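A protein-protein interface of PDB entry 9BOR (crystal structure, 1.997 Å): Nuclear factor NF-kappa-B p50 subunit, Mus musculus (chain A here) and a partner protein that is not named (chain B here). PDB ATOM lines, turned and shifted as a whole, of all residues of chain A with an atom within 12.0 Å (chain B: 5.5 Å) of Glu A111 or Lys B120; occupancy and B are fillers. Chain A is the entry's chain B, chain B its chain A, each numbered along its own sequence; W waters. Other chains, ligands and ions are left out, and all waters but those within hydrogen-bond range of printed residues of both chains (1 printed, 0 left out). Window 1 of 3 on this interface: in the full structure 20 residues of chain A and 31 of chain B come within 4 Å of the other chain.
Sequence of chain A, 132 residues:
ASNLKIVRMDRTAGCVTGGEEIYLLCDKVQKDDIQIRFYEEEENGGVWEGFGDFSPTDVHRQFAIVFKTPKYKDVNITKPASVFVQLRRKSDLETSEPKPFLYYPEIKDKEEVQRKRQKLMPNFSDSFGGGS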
ATOM      1  N   THR A  17     -14.111  -6.913 -10.558  1.00  0.00           N
ATOM      2  CA  THR A  17     -15.161  -7.617  -9.832  1.00  0.00           C
ATOM      3  C   THR A  17     -16.342  -6.712  -9.496  1.00  0.00           C
ATOM      4  O   THR A  17     -17.441  -7.195  -9.241  1.00  0.00           O
ATOM      5  CB  THR A  17     -14.623  -8.227  -8.527  1.00  0.00           C
ATOM      6  OG1 THR A  17     -14.043  -7.193  -7.723  1.00  0.00           O
ATOM      7  CG2 THR A  17     -13.569  -9.274  -8.829  1.00  0.00           C
ATOM      8  N   GLU A 106      -8.352  -8.507 -10.579  1.00  0.00           N
ATOM      9  CA  GLU A 106      -8.456  -8.899  -9.184  1.00  0.00           C
ATOM     10  C   GLU A 106      -7.114  -9.419  -8.690  1.00  0.00           C
ATOM     11  O   GLU A 106      -6.487 -10.258  -9.340  1.00  0.00           O
ATOM     12  CB  GLU A 106      -9.535  -9.965  -9.005  1.00  0.00           C
ATOM     13  CG  GLU A 106      -9.635 -10.503  -7.592  1.00  0.00           C
ATOM     14  CD  GLU A 106     -10.726 -11.541  -7.438  1.00  0.00           C
ATOM     15  OE1 GLU A 106     -11.452 -11.795  -8.423  1.00  0.00           O
ATOM     16  OE2 GLU A 106     -10.859 -12.102  -6.330  1.00  0.00           O
ATOM     17  N   ILE A 107      -6.669  -8.911  -7.547  1.00  0.00           N
ATOM     18  CA  ILE A 107      -5.427  -9.376  -6.949  1.00  0.00           C
ATOM     19  C   ILE A 107      -5.703 -10.547  -6.011  1.00  0.00           C
ATOM     20  O   ILE A 107      -5.976 -10.360  -4.825  1.00  0.00           O
ATOM     21  CB  ILE A 107      -4.698  -8.244  -6.186  1.00  0.00           C
ATOM     22  CG1 ILE A 107      -5.699  -7.361  -5.435  1.00  0.00           C
ATOM     23  CG2 ILE A 107      -3.899  -7.386  -7.152  1.00  0.00           C
ATOM     24  CD1 ILE A 107      -5.055  -6.239  -4.642  1.00  0.00           C
ATOM     25  N   LYS A 108      -5.644 -11.760  -6.554  1.00  0.00           N
ATOM     26  CA  LYS A 108      -5.848 -12.957  -5.749  1.00  0.00           C
ATOM     27  C   LYS A 108      -4.683 -13.141  -4.774  1.00  0.00           C
ATOM     28  O   LYS A 108      -3.544 -12.774  -5.077  1.00  0.00           O
ATOM     29  CB  LYS A 108      -6.003 -14.197  -6.639  1.00  0.00           C
ATOM     30  CG  LYS A 108      -4.714 -14.990  -6.844  1.00  0.00           C
ATOM     31  CD  LYS A 108      -4.974 -16.355  -7.460  1.00  0.00           C
ATOM     32  CE  LYS A 108      -3.719 -17.218  -7.436  1.00  0.00           C
ATOM     33  NZ  LYS A 108      -3.271 -17.511  -6.040  1.00  0.00           N
ATOM     34  N   ASP A 109      -4.989 -13.687  -3.599  1.00  0.00           N
ATOM     35  CA  ASP A 109      -3.988 -14.000  -2.581  1.00  0.00           C
ATOM     36  C   ASP A 109      -3.054 -12.829  -2.280  1.00  0.00           C
ATOM     37  O   ASP A 109      -1.840 -12.923  -2.468  1.00  0.00           O
ATOM     38  CB  ASP A 109      -3.168 -15.223  -3.008  1.00  0.00           C
ATOM     39  CG  ASP A 109      -2.267 -15.741  -1.899  1.00  0.00           C
ATOM     40  OD1 ASP A 109      -2.620 -15.564  -0.713  1.00  0.00           O
ATOM     41  OD2 ASP A 109      -1.207 -16.323  -2.217  1.00  0.00           O
ATOM     42  N   LYS A 110      -3.620 -11.719  -1.816  1.00  0.00           N
ATOM     43  CA  LYS A 110      -2.802 -10.573  -1.447  1.00  0.00           C
ATOM     44  C   LYS A 110      -2.109 -10.832  -0.113  1.00  0.00           C
ATOM     45  O   LYS A 110      -1.147 -10.151   0.242  1.00  0.00           O
ATOM     46  CB  LYS A 110      -3.641  -9.299  -1.375  1.00  0.00           C
ATOM     47  CG  LYS A 110      -4.581  -9.223  -0.193  1.00  0.00           C
ATOM     48  CD  LYS A 110      -5.267  -7.865  -0.158  1.00  0.00           C
ATOM     49  CE  LYS A 110      -6.174  -7.726   1.046  1.00  0.00           C
ATOM     50  NZ  LYS A 110      -6.866  -6.408   1.059  1.00  0.00           N
ATOM     51  N   GLU A 111      -2.598 -11.828   0.619  1.00  0.00           N
ATOM     52  CA  GLU A 111      -1.967 -12.236   1.866  1.00  0.00           C
ATOM     53  C   GLU A 111      -0.704 -13.055   1.591  1.00  0.00           C
ATOM     54  O   GLU A 111       0.047 -13.372   2.512  1.00  0.00           O
ATOM     55  CB  GLU A 111      -2.941 -13.037   2.732  1.00  0.00           C
ATOM     56  CG  GLU A 111      -4.117 -12.228   3.276  1.00  0.00           C
ATOM     57  CD  GLU A 111      -5.265 -12.094   2.286  1.00  0.00           C
ATOM     58  OE1 GLU A 111      -5.192 -12.695   1.195  1.00  0.00           O
ATOM     59  OE2 GLU A 111      -6.245 -11.388   2.608  1.00  0.00           O
ATOM     60  N   GLU A 112      -0.489 -13.382   0.315  1.00  0.00           N
ATOM     61  CA  GLU A 112       0.676 -14.143  -0.146  1.00  0.00           C
ATOM     62  C   GLU A 112       0.754 -15.515   0.512  1.00  0.00           C
ATOM     63  O   GLU A 112       1.837 -15.991   0.852  1.00  0.00           O
ATOM     64  CB  GLU A 112       1.973 -13.357   0.102  1.00  0.00           C
ATOM     65  CG  GLU A 112       2.161 -12.174  -0.841  1.00  0.00           C
ATOM     66  CD  GLU A 112       3.364 -11.315  -0.491  1.00  0.00           C
ATOM     67  OE1 GLU A 112       3.913 -10.664  -1.404  1.00  0.00           O
ATOM     68  OE2 GLU A 112       3.756 -11.279   0.693  1.00  0.00           O
ATOM     69  N   VAL A 113      -0.401 -16.148   0.681  1.00  0.00           N
ATOM     70  CA  VAL A 113      -0.462 -17.480   1.267  1.00  0.00           C
ATOM     71  C   VAL A 113       0.190 -18.501   0.344  1.00  0.00           C
ATOM     72  O   VAL A 113       1.035 -19.286   0.771  1.00  0.00           O
ATOM     73  CB  VAL A 113      -1.916 -17.901   1.557  1.00  0.00           C
ATOM     74  CG1 VAL A 113      -1.976 -19.349   2.017  1.00  0.00           C
ATOM     75  CG2 VAL A 113      -2.530 -16.984   2.602  1.00  0.00           C
ATOM     76  N   GLN A 114      -0.197 -18.474  -0.926  1.00  0.00           N
ATOM     77  CA  GLN A 114       0.321 -19.423  -1.906  1.00  0.00           C
ATOM     78  C   GLN A 114       1.803 -19.202  -2.193  1.00  0.00           C
ATOM     79  O   GLN A 114       2.517 -20.139  -2.550  1.00  0.00           O
ATOM     80  CB  GLN A 114      -0.482 -19.340  -3.205  1.00  0.00           C
ATOM     81  CG  GLN A 114      -1.402 -20.526  -3.424  1.00  0.00           C
ATOM     82  CD  GLN A 114      -0.642 -21.832  -3.546  1.00  0.00           C
ATOM     83  OE1 GLN A 114      -1.008 -22.837  -2.935  1.00  0.00           O
ATOM     84  NE2 GLN A 114       0.423 -21.827  -4.342  1.00  0.00           N
ATOM     85  N   ARG A 115       2.263 -17.965  -2.036  1.00  0.00           N
ATOM     86  CA  ARG A 115       3.671 -17.647  -2.249  1.00  0.00           C
ATOM     87  C   ARG A 115       4.542 -18.309  -1.183  1.00  0.00           C
ATOM     88  O   ARG A 115       5.691 -18.673  -1.437  1.00  0.00           O
ATOM     89  CB  ARG A 115       3.893 -16.134  -2.245  1.00  0.00           C
ATOM     90  CG  ARG A 115       5.326 -15.727  -2.536  1.00  0.00           C
ATOM     91  CD  ARG A 115       5.519 -14.224  -2.451  1.00  0.00           C
ATOM     92  NE  ARG A 115       6.910 -13.852  -2.684  1.00  0.00           N
ATOM     93  CZ  ARG A 115       7.358 -12.603  -2.710  1.00  0.00           C
ATOM     94  NH1 ARG A 115       6.523 -11.590  -2.517  1.00  0.00           N
ATOM     95  NH2 ARG A 115       8.643 -12.363  -2.932  1.00  0.00           N
ATOM     96  N   LYS A 116       3.980 -18.467   0.012  1.00  0.00           N
ATOM     97  CA  LYS A 116       4.695 -19.092   1.118  1.00  0.00           C
ATOM     98  C   LYS A 116       4.680 -20.614   1.025  1.00  0.00           C
ATOM     99  O   LYS A 116       5.624 -21.277   1.454  1.00  0.00           O
ATOM    100  CB  LYS A 116       4.096 -18.649   2.448  1.00  0.00           C
ATOM    101  CG  LYS A 116       4.231 -17.169   2.711  1.00  0.00           C
ATOM    102  CD  LYS A 116       3.241 -16.725   3.766  1.00  0.00           C
ATOM    103  CE  LYS A 116       3.492 -15.291   4.182  1.00  0.00           C
ATOM    104  NZ  LYS A 116       3.469 -14.345   3.038  1.00  0.00           N
ATOM    105  N   ARG A 117       3.603 -21.161   0.468  1.00  0.00           N
ATOM    106  CA  ARG A 117       3.480 -22.605   0.307  1.00  0.00           C
ATOM    107  C   ARG A 117       4.516 -23.138  -0.674  1.00  0.00           C
ATOM    108  O   ARG A 117       4.908 -24.302  -0.604  1.00  0.00           O
ATOM    109  CB  ARG A 117       2.074 -22.978  -0.167  1.00  0.00           C
ATOM    110  CG  ARG A 117       0.973 -22.600   0.805  1.00  0.00           C
ATOM    111  CD  ARG A 117      -0.392 -23.034   0.297  1.00  0.00           C
ATOM    112  NE  ARG A 117      -0.468 -24.477   0.079  1.00  0.00           N
ATOM    113  CZ  ARG A 117      -0.842 -25.355   1.005  1.00  0.00           C
ATOM    114  NH1 ARG A 117      -1.170 -24.939   2.222  1.00  0.00           N
ATOM    115  NH2 ARG A 117      -0.884 -26.649   0.718  1.00  0.00           N
ATOM    116  N   GLN A 118       4.955 -22.278  -1.588  1.00  0.00           N
ATOM    117  CA  GLN A 118       5.938 -22.663  -2.594  1.00  0.00           C
ATOM    118  C   GLN A 118       7.366 -22.580  -2.063  1.00  0.00           C
ATOM    119  O   GLN A 118       8.299 -23.075  -2.697  1.00  0.00           O
ATOM    120  CB  GLN A 118       5.798 -21.787  -3.839  1.00  0.00           C
ATOM    121  CG  GLN A 118       4.464 -21.918  -4.548  1.00  0.00           C
ATOM    122  CD  GLN A 118       4.522 -21.418  -5.977  1.00  0.00           C
ATOM    123  OE1 GLN A 118       5.249 -20.474  -6.286  1.00  0.00           O
ATOM    124  NE2 GLN A 118       3.756 -22.051  -6.858  1.00  0.00           N
ATOM    125  N   LYS A 119       7.535 -21.953  -0.903  1.00  0.00           N
ATOM    126  CA  LYS A 119       8.856 -21.818  -0.301  1.00  0.00           C
ATOM    127  C   LYS A 119       9.355 -23.151   0.243  1.00  0.00           C
ATOM    128  O   LYS A 119       8.567 -24.070   0.473  1.00  0.00           O
ATOM    129  CB  LYS A 119       8.836 -20.768   0.811  1.00  0.00           C
ATOM    130  CG  LYS A 119       8.559 -19.360   0.322  1.00  0.00           C
ATOM    131  CD  LYS A 119       8.716 -18.348   1.445  1.00  0.00           C
ATOM    132  CE  LYS A 119       8.441 -16.934   0.956  1.00  0.00           C
ATOM    133  NZ  LYS A 119       8.638 -15.923   2.033  1.00  0.00           N
ATOM    134  N   GLU B  74       5.454 -10.397   9.297  1.00  0.00           N
ATOM    135  CA  GLU B  74       6.119 -10.292   8.004  1.00  0.00           C
ATOM    136  C   GLU B  74       5.971  -8.892   7.411  1.00  0.00           C
ATOM    137  O   GLU B  74       5.535  -7.960   8.091  1.00  0.00           O
ATOM    138  CB  GLU B  74       5.538 -11.313   7.036  1.00  0.00           C
ATOM    139  CG  GLU B  74       4.098 -11.001   6.652  1.00  0.00           C
ATOM    140  CD  GLU B  74       3.482 -12.105   5.844  1.00  0.00           C
ATOM    141  OE1 GLU B  74       3.411 -13.233   6.370  1.00  0.00           O
ATOM    142  OE2 GLU B  74       3.085 -11.850   4.687  1.00  0.00           O
ATOM    143  N   ASN B  76       3.849  -7.928   5.353  1.00  0.00           N
ATOM    144  CA  ASN B  76       2.427  -7.603   5.232  1.00  0.00           C
ATOM    145  C   ASN B  76       1.779  -7.262   6.573  1.00  0.00           C
ATOM    146  O   ASN B  76       0.569  -7.040   6.648  1.00  0.00           O
ATOM    147  CB  ASN B  76       1.668  -8.762   4.582  1.00  0.00           C
ATOM    148  CG  ASN B  76       1.951  -8.887   3.098  1.00  0.00           C
ATOM    149  OD1 ASN B  76       1.932  -7.895   2.365  1.00  0.00           O
ATOM    150  ND2 ASN B  76       2.223 -10.108   2.646  1.00  0.00           N
ATOM    151  N   GLN B  78       1.643  -9.314   9.009  1.00  0.00           N
ATOM    152  CA  GLN B  78       0.980 -10.542   9.437  1.00  0.00           C
ATOM    153  C   GLN B  78       1.837 -11.418  10.347  1.00  0.00           C
ATOM    154  O   GLN B  78       2.924 -11.855   9.963  1.00  0.00           O
ATOM    155  CB  GLN B  78       0.564 -11.361   8.218  1.00  0.00           C
ATOM    156  CG  GLN B  78      -0.456 -10.689   7.334  1.00  0.00           C
ATOM    157  CD  GLN B  78      -0.715 -11.472   6.070  1.00  0.00           C
ATOM    158  OE1 GLN B  78       0.212 -11.997   5.451  1.00  0.00           O
ATOM    159  NE2 GLN B  78      -1.980 -11.570   5.685  1.00  0.00           N
ATOM    160  N   VAL B  85      -4.972 -17.709   9.660  1.00  0.00           N
ATOM    161  CA  VAL B  85      -6.328 -17.229   9.414  1.00  0.00           C
ATOM    162  C   VAL B  85      -6.585 -17.148   7.918  1.00  0.00           C
ATOM    163  O   VAL B  85      -7.520 -17.762   7.404  1.00  0.00           O
ATOM    164  CB  VAL B  85      -6.562 -15.852  10.049  1.00  0.00           C
ATOM    165  CG1 VAL B  85      -7.931 -15.301   9.644  1.00  0.00           C
ATOM    166  CG2 VAL B  85      -6.432 -15.938  11.563  1.00  0.00           C
ATOM    167  N   ALA B  86      -5.728 -16.411   7.220  1.00  0.00           N
ATOM    168  CA  ALA B  86      -5.871 -16.226   5.782  1.00  0.00           C
ATOM    169  C   ALA B  86      -5.789 -17.551   5.040  1.00  0.00           C
ATOM    170  O   ALA B  86      -6.461 -17.748   4.029  1.00  0.00           O
ATOM    171  CB  ALA B  86      -4.811 -15.262   5.263  1.00  0.00           C
ATOM    172  N   TRP B 109      -3.142  -3.653   5.953  1.00  0.00           N
ATOM    173  CA  TRP B 109      -4.317  -3.083   5.307  1.00  0.00           C
ATOM    174  C   TRP B 109      -5.370  -2.664   6.330  1.00  0.00           C
ATOM    175  O   TRP B 109      -6.450  -2.205   5.965  1.00  0.00           O
ATOM    176  CB  TRP B 109      -4.911  -4.078   4.309  1.00  0.00           C
ATOM    177  CG  TRP B 109      -3.933  -4.516   3.271  1.00  0.00           C
ATOM    178  CD1 TRP B 109      -3.522  -3.807   2.179  1.00  0.00           C
ATOM    179  CD2 TRP B 109      -3.236  -5.768   3.223  1.00  0.00           C
ATOM    180  NE1 TRP B 109      -2.612  -4.539   1.454  1.00  0.00           N
ATOM    181  CE2 TRP B 109      -2.422  -5.748   2.071  1.00  0.00           C
ATOM    182  CE3 TRP B 109      -3.222  -6.905   4.039  1.00  0.00           C
ATOM    183  CZ2 TRP B 109      -1.601  -6.819   1.717  1.00  0.00           C
ATOM    184  CZ3 TRP B 109      -2.412  -7.966   3.686  1.00  0.00           C
ATOM    185  CH2 TRP B 109      -1.611  -7.916   2.535  1.00  0.00           C
ATOM    186  N   ARG B 111      -6.894  -4.599   8.575  1.00  0.00           N
ATOM    187  CA  ARG B 111      -7.870  -5.641   8.882  1.00  0.00           C
ATOM    188  C   ARG B 111      -7.465  -6.468  10.097  1.00  0.00           C
ATOM    189  O   ARG B 111      -6.306  -6.877  10.219  1.00  0.00           O
ATOM    190  CB  ARG B 111      -8.051  -6.565   7.678  1.00  0.00           C
ATOM    191  CG  ARG B 111      -7.975  -5.857   6.336  1.00  0.00           C
ATOM    192  CD  ARG B 111      -7.192  -6.695   5.337  1.00  0.00           C
ATOM    193  NE  ARG B 111      -7.995  -7.750   4.732  1.00  0.00           N
ATOM    194  CZ  ARG B 111      -7.497  -8.863   4.203  1.00  0.00           C
ATOM    195  NH1 ARG B 111      -6.190  -9.092   4.229  1.00  0.00           N
ATOM    196  NH2 ARG B 111      -8.310  -9.759   3.666  1.00  0.00           N
ATOM    197  N   HIS B 115     -11.851  -9.623  10.730  1.00  0.00           N
ATOM    198  CA  HIS B 115     -12.223  -9.035   9.442  1.00  0.00           C
ATOM    199  C   HIS B 115     -11.871  -9.986   8.306  1.00  0.00           C
ATOM    200  O   HIS B 115     -12.649 -10.158   7.372  1.00  0.00           O
ATOM    201  CB  HIS B 115     -11.536  -7.680   9.226  1.00  0.00           C
ATOM    202  CG  HIS B 115     -12.117  -6.568  10.041  1.00  0.00           C
ATOM    203  ND1 HIS B 115     -11.511  -6.084  11.184  1.00  0.00           N
ATOM    204  CD2 HIS B 115     -13.246  -5.837   9.880  1.00  0.00           C
ATOM    205  CE1 HIS B 115     -12.243  -5.111  11.691  1.00  0.00           C
ATOM    206  NE2 HIS B 115     -13.305  -4.940  10.919  1.00  0.00           N
ATOM    207  N   VAL B 116     -10.699 -10.607   8.381  1.00  0.00           N
ATOM    208  CA  VAL B 116     -10.292 -11.540   7.336  1.00  0.00           C
ATOM    209  C   VAL B 116     -11.211 -12.763   7.313  1.00  0.00           C
ATOM    210  O   VAL B 116     -11.612 -13.228   6.244  1.00  0.00           O
ATOM    211  CB  VAL B 116      -8.834 -11.999   7.512  1.00  0.00           C
ATOM    212  CG1 VAL B 116      -8.464 -12.960   6.404  1.00  0.00           C
ATOM    213  CG2 VAL B 116      -7.892 -10.802   7.509  1.00  0.00           C
ATOM    214  N   CYS B 117     -11.539 -13.280   8.495  1.00  0.00           N
ATOM    215  CA  CYS B 117     -12.521 -14.362   8.616  1.00  0.00           C
ATOM    216  C   CYS B 117     -13.839 -13.977   7.967  1.00  0.00           C
ATOM    217  O   CYS B 117     -14.424 -14.739   7.195  1.00  0.00           O
ATOM    218  CB  CYS B 117     -12.776 -14.713  10.082  1.00  0.00           C
ATOM    219  SG  CYS B 117     -11.458 -15.626  10.873  1.00  0.00           S
ATOM    220  N   ALA B 118     -14.290 -12.773   8.293  1.00  0.00           N
ATOM    221  CA  ALA B 118     -15.571 -12.271   7.827  1.00  0.00           C
ATOM    222  C   ALA B 118     -15.630 -12.169   6.308  1.00  0.00           C
ATOM    223  O   ALA B 118     -16.606 -12.595   5.690  1.00  0.00           O
ATOM    224  CB  ALA B 118     -15.854 -10.921   8.459  1.00  0.00           C
ATOM    225  N   GLU B 119     -14.581 -11.606   5.712  1.00  0.00           N
ATOM    226  CA  GLU B 119     -14.518 -11.418   4.267  1.00  0.00           C
ATOM    227  C   GLU B 119     -14.511 -12.738   3.514  1.00  0.00           C
ATOM    228  O   GLU B 119     -15.130 -12.864   2.455  1.00  0.00           O
ATOM    229  CB  GLU B 119     -13.266 -10.622   3.877  1.00  0.00           C
ATOM    230  CG  GLU B 119     -13.254  -9.171   4.323  1.00  0.00           C
ATOM    231  CD  GLU B 119     -11.991  -8.449   3.878  1.00  0.00           C
ATOM    232  OE1 GLU B 119     -11.800  -7.278   4.272  1.00  0.00           O
ATOM    233  OE2 GLU B 119     -11.188  -9.055   3.135  1.00  0.00           O
ATOM    234  N   LYS B 120     -13.790 -13.715   4.056  1.00  0.00           N
ATOM    235  CA  LYS B 120     -13.547 -14.971   3.353  1.00  0.00           C
ATOM    236  C   LYS B 120     -14.508 -16.074   3.765  1.00  0.00           C
ATOM    237  O   LYS B 120     -14.525 -17.141   3.157  1.00  0.00           O
ATOM    238  CB  LYS B 120     -12.103 -15.433   3.580  1.00  0.00           C
ATOM    239  CG  LYS B 120     -11.060 -14.482   3.014  1.00  0.00           C
ATOM    240  CD  LYS B 120      -9.653 -15.042   3.167  1.00  0.00           C
ATOM    241  CE  LYS B 120      -8.607 -14.088   2.599  1.00  0.00           C
ATOM    242  NZ  LYS B 120      -8.820 -13.808   1.153  1.00  0.00           N
ATOM    243  N   GLY B 121     -15.305 -15.821   4.797  1.00  0.00           N
ATOM    244  CA  GLY B 121     -16.267 -16.805   5.256  1.00  0.00           C
ATOM    245  C   GLY B 121     -15.631 -17.998   5.951  1.00  0.00           C
ATOM    246  O   GLY B 121     -16.141 -19.117   5.864  1.00  0.00           O
ATOM    247  N   HIS B 122     -14.525 -17.756   6.651  1.00  0.00           N
ATOM    248  CA  HIS B 122     -13.822 -18.810   7.383  1.00  0.00           C
ATOM    249  C   HIS B 122     -14.415 -19.016   8.774  1.00  0.00           C
ATOM    250  O   HIS B 122     -13.836 -18.590   9.773  1.00  0.00           O
ATOM    251  CB  HIS B 122     -12.329 -18.483   7.508  1.00  0.00           C
ATOM    252  CG  HIS B 122     -11.590 -18.506   6.204  1.00  0.00           C
ATOM    253  ND1 HIS B 122     -10.291 -18.064   6.080  1.00  0.00           N
ATOM    254  CD2 HIS B 122     -11.964 -18.925   4.972  1.00  0.00           C
ATOM    255  CE1 HIS B 122      -9.896 -18.205   4.826  1.00  0.00           C
ATOM    256  NE2 HIS B 122     -10.893 -18.727   4.134  1.00  0.00           N
ATOM    257  N   LYS B 184     -19.650 -20.539  -0.716  1.00  0.00           N
ATOM    258  CA  LYS B 184     -19.334 -19.292  -0.030  1.00  0.00           C
ATOM    259  C   LYS B 184     -20.613 -18.647   0.514  1.00  0.00           C
ATOM    260  O   LYS B 184     -20.593 -17.987   1.555  1.00  0.00           O
ATOM    261  CB  LYS B 184     -18.598 -18.336  -0.966  1.00  0.00           C
ATOM    262  CG  LYS B 184     -17.565 -17.470  -0.263  1.00  0.00           C
ATOM    263  CD  LYS B 184     -16.739 -16.680  -1.264  1.00  0.00           C
ATOM    264  CE  LYS B 184     -15.710 -15.804  -0.567  1.00  0.00           C
ATOM    265  NZ  LYS B 184     -14.873 -15.057  -1.546  1.00  0.00           N
ATOM    266  N   SER B 187     -20.954 -20.594   3.701  1.00  0.00           N
ATOM    267  CA  SER B 187     -19.898 -20.307   4.668  1.00  0.00           C
ATOM    268  C   SER B 187     -20.004 -18.898   5.247  1.00  0.00           C
ATOM    269  O   SER B 187     -19.724 -18.682   6.428  1.00  0.00           O
ATOM    270  CB  SER B 187     -18.518 -20.507   4.030  1.00  0.00           C
ATOM    271  OG  SER B 187     -18.266 -19.537   3.027  1.00  0.00           O
ATOM    272  N   LEU B 188     -20.406 -17.938   4.420  1.00  0.00           N
ATOM    273  CA  LEU B 188     -20.544 -16.560   4.883  1.00  0.00           C
ATOM    274  C   LEU B 188     -21.682 -16.434   5.895  1.00  0.00           C
ATOM    275  O   LEU B 188     -21.569 -15.697   6.875  1.00  0.00           O
ATOM    276  CB  LEU B 188     -20.762 -15.612   3.701  1.00  0.00           C
ATOM    277  CG  LEU B 188     -19.479 -15.270   2.938  1.00  0.00           C
ATOM    278  CD1 LEU B 188     -19.781 -14.578   1.621  1.00  0.00           C
ATOM    279  CD2 LEU B 188     -18.562 -14.412   3.811  1.00  0.00           C
HETATM  280  O   HOH W   1      -7.084 -12.822  -1.233  1.00  0.00           O
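The side-chain amide nitrogen of Asn B76 is in hydrogen-bond range of the side-chain carboxylate of Glu A112, 2.7 Å away. O of Glu A111 lies close to OE1 of Gln B78. The side-chain carboxylate (OE2) of Glu B74 is in salt-bridge range of the side-chain amino group (NZ) of Lys A116. NH1 of Arg B111 lies within salt-bridge range of OE2 of Glu A111. The side-chain amino group (NZ) of Lys B120 lies within salt-bridge range of the side-chain carboxylate (OE1) of Glu A111 (3.8 Å).
NH2 of Arg B111 is in salt-bridge range of OE2 of Glu B119, at 3.0 Å. OE2 of Glu B74 lies close to OE1 of Gln B78 (3.0 Å). The backbone NH (N) of Glu A112 is in hydrogen-bond range of the side-chain carboxylate (OD1) of Asp A109, 3.2 Å away. OD1 of Asp A109 is in hydrogen-bond range of N of Val A113 (2.7 Å). The side-chain carboxylate of Glu A112 is in salt-bridge range of the guanidinium group of Arg A115 (3.0 Å). The side-chain carboxylate of Glu A112 lies within salt-bridge range of the side-chain amino group of Lys A116.
CH2 of Trp B109 touches O of Lys A110 (3.2 Å). CE of Lys A110 touches NH1 of Arg B111, at 3.5 Å. Glu A111 touches Asn B76. Ala B86 touches Glu A111 (CB to CG, 3.7 Å). CG2 of Val A113 touches CB of Ala B86 (3.9 Å).
Of chain B, only Asn B76 (3.9 Å), Gln B78 (3.2 Å), Ala B86 (3.7 Å), Arg B111 (2.8 Å) and Lys B120 (3.6 Å) come within 4 Å of Glu A111. Lys B120 touches just one residue of chain A: Glu A111 (3.6 Å). Of chain A, only Glu A111 and Glu A112 come within 4 Å of Asn B76. Of chain A, only Glu A111 (3.7 Å) and Val A113 (3.9 Å) come within 4 Å of Ala B86. No residue of chain A comes within 4 Å of Glu B119. No residue of chain A comes within 4 Å of Gly B121. No residue of chain A comes within 4 Å of Lys B184. No residue of chain A comes within 4 Å of Leu B188. Printed residues of chain B within 4 Å of Glu A112: Asn B76. Of the printed residues of chain A, Glu B74 touches Lys A116. Of the printed residues of chain A, Trp B109 touches Lys A110. Printed residues of chain B within 4 Å of Lys A116: Glu B74. Ile A107 touches none of the printed residues of chain B. The nearest residue of chain B that does not touch Glu A111 is Glu B74 (4.03 Å). The nearest residue of chain A that does not touch Lys B120 is Asp A109 (6.1 Å). The nearest printed residue of chain B that does not touch Val A113 is Gln B78 (6.3 Å).
Of the 18 printed residues of chain B, 7 touch a printed residue of chain A. Hydrophobic or aromatic side chains of chain B that line the printed part of chain A: Ala B86 and Trp B109. Along chain B the printed residues that touch a printed residue of chain A span positions 74 to 120. Of the 15 printed residues of chain A, 5 touch a printed residue of chain B. Hydrophobic or aromatic side chains of chain A within 4 Å of the printed part of chain B: Val A113. Among the printed residues, 10 pairs touch across the chains. Among the printed residues, Asp or Glu carboxylates within 4 Å of a Lys or Arg side-chain nitrogen of the other chain: Glu A111 with Arg B111, Glu A111 with Lys B120 and Lys A116 with Glu B74.
Water W1 lies within hydrogen-bond range of OE1 of Glu A111 (3.1 Å), NZ of Lys B120 (3.1 Å) and N of Asp A109 (3.3 Å).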
